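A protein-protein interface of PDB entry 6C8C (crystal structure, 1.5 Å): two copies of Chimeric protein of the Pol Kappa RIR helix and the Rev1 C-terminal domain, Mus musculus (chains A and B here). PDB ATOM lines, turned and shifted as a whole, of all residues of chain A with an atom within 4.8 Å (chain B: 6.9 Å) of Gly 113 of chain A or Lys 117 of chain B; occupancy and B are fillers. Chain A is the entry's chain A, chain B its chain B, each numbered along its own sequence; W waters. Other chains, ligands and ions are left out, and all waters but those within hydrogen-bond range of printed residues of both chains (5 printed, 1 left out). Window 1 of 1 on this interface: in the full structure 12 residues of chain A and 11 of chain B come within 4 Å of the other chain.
O of Gly 113 of chain A lies within hydrogen-bond range of NZ of Lys 117 of chain B, 2.7 Å away. The backbone carbonyl oxygen (O) of Thr 115 of chain A lies within hydrogen-bond range of the backbone NH (N) of Lys 117 of chain B (2.9 Å). The backbone NH (N) of Lys 117 of chain A is in hydrogen-bond range of the backbone carbonyl oxygen (O) of Thr 115 of chain B, 2.8 Å away.
The side-chain amino group (NZ) of Lys 79 of chain B is in salt-bridge range of the side-chain carboxylate (OD2) of Asp 75 of chain B, 2.8 Å away. The side-chain amino group of Lys 79 of chain B lies within salt-bridge range of the chain-end carboxylate of Thr 119 of chain B, at 3.9 Å. N of Leu 116 of chain B lies within hydrogen-bond range of OE1 of Gln 105 of chain B (2.8 Å).
Among the printed residues, merely in contact across the chains: Leu 116 of chain A with Thr 115 of chain B, Thr 115 of chain A with Leu 116 of chain B, Leu 116 of chain A with Lys 117 of chain B, Thr 115 of chain A with Asp 75 of chain B, Ser 114 of chain A with Lys 117 of chain B, Lys 117 of chain A with Lys 117 of chain B, Ser 114 of chain A with Thr 119 of chain B and Thr 115 of chain A with Thr 115 of chain B.
Tyr 112 of chain A touches none of the printed residues of chain B. Gly 113 of chain A touches just one residue of chain B: Lys 117. Printed residues of chain A within 4 Å of Asp 75 of chain B: Thr 115. Printed residues of chain A within 4 Å of Thr 115 of chain B: Thr 115 (3.99 Å), Leu 116 (3.4 Å) and Lys 117 (2.8 Å). Printed residues of chain A within 4 Å of Leu 116 of chain B: Thr 115 (3.4 Å). Of chain A, only Gly 113 (2.7 Å), Ser 114 (3.9 Å), Thr 115 (2.9 Å), Leu 116 (3.5 Å) and Lys 117 (3.9 Å) come within 4 Å of Lys 117 of chain B. The nearest printed residue of chain B that does not touch Leu 116 of chain A is Leu 116 of chain B (4.2 Å).
Of the 8 printed residues of chain B, 5 touch a printed residue of chain A. Printed residues of chain B that touch a printed residue of chain A: Asp 75, Thr 115, Leu 116, Lys 117 and Thr 119. Among the printed residues, 11 pairs touch across the chains.
Thr 115 of chain B touches its own counterpart, Thr 115 of chain A. Thr 115 of chain A touches Leu 116 of chain B, and with the chains exchanged Leu 116 of chain A touches Thr 115 of chain B. Thr 115 of chain A touches Lys 117 of chain B, and with the chains exchanged Lys 117 of chain A touches Thr 115 of chain B. Leu 116 of chain A touches Lys 117 of chain B, but with the chains exchanged Lys 117 of chain A does not touch Leu 116 of chain B (4.9 Å). Positions printed for both chains: 115, 116 and 117.
Water W2 lies within hydrogen-bond range of the side-chain carboxylate of Asp 75 of chain B, the backbone carbonyl oxygen of Thr 115 of chain A, the backbone NH of Val 118 of chain B and the backbone NH of Lys 117 of chain B. Water W3 lies within hydrogen-bond range of the side-chain hydroxyl (OG1) of Thr 119 of chain B (2.6 Å) and the backbone carbonyl oxygen (O) of Ser 114 of chain A (2.8 Å). Water W1 lies within hydrogen-bond range of OG1 of Thr 115 of chain B (2.6 Å) and O of Lys 117 of chain A (2.9 Å). Water W5 lies within hydrogen-bond range of the side-chain hydroxyl of Ser 114 of chain A, the side-chain hydroxyl of Thr 115 of chain A and the side-chain amino group of Lys 79 of chain B. Water W4 bridges the side-chain amino group (NZ) of Lys 117 of chain B (3.1 Å) and the backbone carbonyl oxygen (O) of Gly 113 of chain A (3.4 Å).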
ATOM      1  N   GLN A 109      29.841   6.122   9.849  1.00  0.00           N
ATOM      2  CA  GLN A 109      29.372   5.478   8.632  1.00  0.00           C
ATOM      3  C   GLN A 109      30.364   4.431   8.157  1.00  0.00           C
ATOM      4  O   GLN A 109      29.976   3.315   7.789  1.00  0.00           O
ATOM      5  CB  GLN A 109      29.130   6.533   7.550  1.00  0.00           C
ATOM      6  CG  GLN A 109      28.750   5.977   6.187  1.00  0.00           C
ATOM      7  CD  GLN A 109      29.955   5.673   5.333  1.00  0.00           C
ATOM      8  OE1 GLN A 109      30.817   6.528   5.145  1.00  0.00           O
ATOM      9  NE2 GLN A 109      30.021   4.451   4.798  1.00  0.00           N
ATOM     10  N   GLN A 110      31.653   4.759   8.178  1.00  0.00           N
ATOM     11  CA  GLN A 110      32.646   3.798   7.710  1.00  0.00           C
ATOM     12  C   GLN A 110      32.802   2.636   8.682  1.00  0.00           C
ATOM     13  O   GLN A 110      32.936   1.482   8.257  1.00  0.00           O
ATOM     14  CB  GLN A 110      33.980   4.506   7.484  1.00  0.00           C
ATOM     15  CG  GLN A 110      33.880   5.566   6.408  1.00  0.00           C
ATOM     16  CD  GLN A 110      35.191   6.233   6.099  1.00  0.00           C
ATOM     17  OE1 GLN A 110      36.061   6.377   6.969  1.00  0.00           O
ATOM     18  NE2 GLN A 110      35.337   6.661   4.849  1.00  0.00           N
ATOM     19  N   THR A 111      32.806   2.917   9.990  1.00  0.00           N
ATOM     20  CA  THR A 111      32.899   1.843  10.971  1.00  0.00           C
ATOM     21  C   THR A 111      31.785   0.829  10.775  1.00  0.00           C
ATOM     22  O   THR A 111      32.009  -0.388  10.866  1.00  0.00           O
ATOM     23  CB  THR A 111      32.836   2.428  12.378  1.00  0.00           C
ATOM     24  OG1 THR A 111      33.949   3.308  12.557  1.00  0.00           O
ATOM     25  CG2 THR A 111      32.859   1.320  13.445  1.00  0.00           C
ATOM     26  N   TYR A 112      30.575   1.312  10.495  1.00  0.00           N
ATOM     27  CA  TYR A 112      29.419   0.462  10.239  1.00  0.00           C
ATOM     28  C   TYR A 112      29.091   0.376   8.756  1.00  0.00           C
ATOM     29  O   TYR A 112      27.928   0.216   8.380  1.00  0.00           O
ATOM     30  CB  TYR A 112      28.225   0.964  11.050  1.00  0.00           C
ATOM     31  CG  TYR A 112      28.452   0.749  12.520  1.00  0.00           C
ATOM     32  CD1 TYR A 112      28.407  -0.532  13.058  1.00  0.00           C
ATOM     33  CD2 TYR A 112      28.732   1.806  13.373  1.00  0.00           C
ATOM     34  CE1 TYR A 112      28.633  -0.755  14.398  1.00  0.00           C
ATOM     35  CE2 TYR A 112      28.952   1.591  14.724  1.00  0.00           C
ATOM     36  CZ  TYR A 112      28.906   0.306  15.228  1.00  0.00           C
ATOM     37  OH  TYR A 112      29.123   0.080  16.567  1.00  0.00           O
ATOM     38  N   GLY A 113      30.121   0.435   7.908  1.00  0.00           N
ATOM     39  CA  GLY A 113      29.903   0.394   6.473  1.00  0.00           C
ATOM     40  C   GLY A 113      29.181  -0.851   6.001  1.00  0.00           C
ATOM     41  O   GLY A 113      28.425  -0.794   5.031  1.00  0.00           O
ATOM     42  N   SER A 114      29.402  -1.983   6.667  1.00  0.00           N
ATOM     43  CA  SER A 114      28.763  -3.225   6.257  1.00  0.00           C
ATOM     44  C   SER A 114      27.368  -3.382   6.833  1.00  0.00           C
ATOM     45  O   SER A 114      26.640  -4.284   6.401  1.00  0.00           O
ATOM     46  CB  SER A 114      29.605  -4.432   6.683  1.00  0.00           C
ATOM     47  OG  SER A 114      29.539  -4.607   8.096  1.00  0.00           O
ATOM     48  N   THR A 115      26.989  -2.529   7.783  1.00  0.00           N
ATOM     49  CA  THR A 115      25.734  -2.625   8.515  1.00  0.00           C
ATOM     50  C   THR A 115      24.720  -1.563   8.122  1.00  0.00           C
ATOM     51  O   THR A 115      23.518  -1.858   8.050  1.00  0.00           O
ATOM     52  CB  THR A 115      26.019  -2.528  10.026  1.00  0.00           C
ATOM     53  OG1 THR A 115      26.881  -3.606  10.420  1.00  0.00           O
ATOM     54  CG2 THR A 115      24.741  -2.589  10.850  1.00  0.00           C
ATOM     55  N   LEU A 116      25.161  -0.330   7.882  1.00  0.00           N
ATOM     56  CA  LEU A 116      24.276   0.810   7.705  1.00  0.00           C
ATOM     57  C   LEU A 116      24.391   1.367   6.297  1.00  0.00           C
ATOM     58  O   LEU A 116      25.483   1.423   5.723  1.00  0.00           O
ATOM     59  CB  LEU A 116      24.603   1.939   8.687  1.00  0.00           C
ATOM     60  CG  LEU A 116      24.332   1.703  10.160  1.00  0.00           C
ATOM     61  CD1 LEU A 116      24.761   2.930  10.936  1.00  0.00           C
ATOM     62  CD2 LEU A 116      22.856   1.391  10.371  1.00  0.00           C
ATOM     63  N   LYS A 117      23.256   1.795   5.760  1.00  0.00           N
ATOM     64  CA  LYS A 117      23.208   2.547   4.515  1.00  0.00           C
ATOM     65  C   LYS A 117      22.703   3.944   4.852  1.00  0.00           C
ATOM     66  O   LYS A 117      21.595   4.100   5.371  1.00  0.00           O
ATOM     67  CB  LYS A 117      22.306   1.846   3.500  1.00  0.00           C
ATOM     68  CG  LYS A 117      22.010   2.660   2.254  1.00  0.00           C
ATOM     69  N   ASP B  75      21.474  -5.726  14.632  1.00  0.00           N
ATOM     70  CA  ASP B  75      21.826  -6.356  13.365  1.00  0.00           C
ATOM     71  C   ASP B  75      21.833  -7.879  13.481  1.00  0.00           C
ATOM     72  O   ASP B  75      21.317  -8.573  12.597  1.00  0.00           O
ATOM     73  CB  ASP B  75      23.178  -5.826  12.898  1.00  0.00           C
ATOM     74  CG  ASP B  75      23.443  -6.106  11.439  1.00  0.00           C
ATOM     75  OD1 ASP B  75      22.609  -5.732  10.594  1.00  0.00           O
ATOM     76  OD2 ASP B  75      24.511  -6.692  11.157  1.00  0.00           O
ATOM     77  N   LYS B  79      19.143 -10.211  11.360  1.00  0.00           N
ATOM     78  CA  LYS B  79      19.647 -11.198  10.409  1.00  0.00           C
ATOM     79  C   LYS B  79      19.305 -12.625  10.820  1.00  0.00           C
ATOM     80  O   LYS B  79      19.111 -13.486   9.949  1.00  0.00           O
ATOM     81  CB  LYS B  79      21.161 -11.020  10.245  1.00  0.00           C
ATOM     82  CG  LYS B  79      21.513  -9.772   9.457  1.00  0.00           C
ATOM     83  CD  LYS B  79      22.991  -9.480   9.479  1.00  0.00           C
ATOM     84  CE  LYS B  79      23.287  -8.368   8.520  1.00  0.00           C
ATOM     85  NZ  LYS B  79      24.701  -7.924   8.653  1.00  0.00           N
ATOM     86  N   GLN B 105      13.162  -0.162  10.012  1.00  0.00           N
ATOM     87  CA  GLN B 105      13.801   0.760   9.069  1.00  0.00           C
ATOM     88  C   GLN B 105      13.206   2.159   9.151  1.00  0.00           C
ATOM     89  O   GLN B 105      13.934   3.144   8.959  1.00  0.00           O
ATOM     90  CB  GLN B 105      13.679   0.235   7.632  1.00  0.00           C
ATOM     91  CG  GLN B 105      14.307  -1.124   7.363  1.00  0.00           C
ATOM     92  CD  GLN B 105      15.834  -1.084   7.304  1.00  0.00           C
ATOM     93  OE1 GLN B 105      16.499  -0.603   8.228  1.00  0.00           O
ATOM     94  NE2 GLN B 105      16.397  -1.605   6.213  1.00  0.00           N
ATOM     95  N   THR B 115      19.554   3.306   7.366  1.00  0.00           N
ATOM     96  CA  THR B 115      18.798   2.066   7.467  1.00  0.00           C
ATOM     97  C   THR B 115      19.781   0.905   7.472  1.00  0.00           C
ATOM     98  O   THR B 115      20.960   1.063   7.134  1.00  0.00           O
ATOM     99  CB  THR B 115      17.794   1.884   6.313  1.00  0.00           C
ATOM    100  OG1 THR B 115      18.475   1.986   5.059  1.00  0.00           O
ATOM    101  CG2 THR B 115      16.700   2.935   6.368  1.00  0.00           C
ATOM    102  N   LEU B 116      19.290  -0.269   7.864  1.00  0.00           N
ATOM    103  CA  LEU B 116      20.107  -1.478   7.834  1.00  0.00           C
ATOM    104  C   LEU B 116      20.263  -1.987   6.411  1.00  0.00           C
ATOM    105  O   LEU B 116      19.295  -2.036   5.646  1.00  0.00           O
ATOM    106  CB  LEU B 116      19.483  -2.583   8.693  1.00  0.00           C
ATOM    107  CG  LEU B 116      19.333  -2.315  10.186  1.00  0.00           C
ATOM    108  CD1 LEU B 116      18.580  -3.467  10.826  1.00  0.00           C
ATOM    109  CD2 LEU B 116      20.700  -2.166  10.822  1.00  0.00           C
ATOM    110  N   LYS B 117      21.492  -2.390   6.072  1.00  0.00           N
ATOM    111  CA  LYS B 117      21.754  -3.060   4.798  1.00  0.00           C
ATOM    112  C   LYS B 117      21.244  -4.494   4.798  1.00  0.00           C
ATOM    113  O   LYS B 117      20.844  -5.003   3.743  1.00  0.00           O
ATOM    114  CB  LYS B 117      23.251  -3.066   4.498  1.00  0.00           C
ATOM    115  CG  LYS B 117      23.817  -1.746   4.024  1.00  0.00           C
ATOM    116  CD  LYS B 117      25.269  -1.903   3.611  1.00  0.00           C
ATOM    117  CE  LYS B 117      25.761  -0.647   2.923  1.00  0.00           C
ATOM    118  NZ  LYS B 117      27.215  -0.729   2.570  1.00  0.00           N
ATOM    119  N   VAL B 118      21.271  -5.160   5.957  1.00  0.00           N
ATOM    120  CA  VAL B 118      20.892  -6.569   6.107  1.00  0.00           C
ATOM    121  C   VAL B 118      21.539  -7.426   5.016  1.00  0.00           C
ATOM    122  O   VAL B 118      20.866  -8.228   4.355  1.00  0.00           O
ATOM    123  CB  VAL B 118      19.356  -6.758   6.112  1.00  0.00           C
ATOM    124  CG1 VAL B 118      18.982  -8.111   6.741  1.00  0.00           C
ATOM    125  CG2 VAL B 118      18.661  -5.655   6.873  1.00  0.00           C
ATOM    126  N   THR B 119      22.845  -7.276   4.813  1.00  0.00           N
ATOM    127  CA  THR B 119      23.523  -8.151   3.859  1.00  0.00           C
ATOM    128  C   THR B 119      24.473  -9.091   4.589  1.00  0.00           C
ATOM    129  O   THR B 119      24.017  -9.935   5.369  1.00  0.00           O
ATOM    130  CB  THR B 119      24.287  -7.359   2.779  1.00  0.00           C
ATOM    131  OG1 THR B 119      24.992  -6.272   3.383  1.00  0.00           O
ATOM    132  CG2 THR B 119      23.321  -6.811   1.735  1.00  0.00           C
ATOM    133  OXT THR B 119      25.693  -9.040   4.421  1.00  0.00           O
HETATM  134  O   HOH W   1      19.119   4.277   3.935  1.00  0.00           O
HETATM  135  O   HOH W   2      22.681  -4.516   8.317  1.00  0.00           O
HETATM  136  O   HOH W   3      27.412  -6.034   4.373  1.00  0.00           O
HETATM  137  O   HOH W   4      29.082   1.696   2.849  1.00  0.00           O
HETATM  138  O   HOH W   5      27.344  -6.159   9.065  1.00  0.00           O
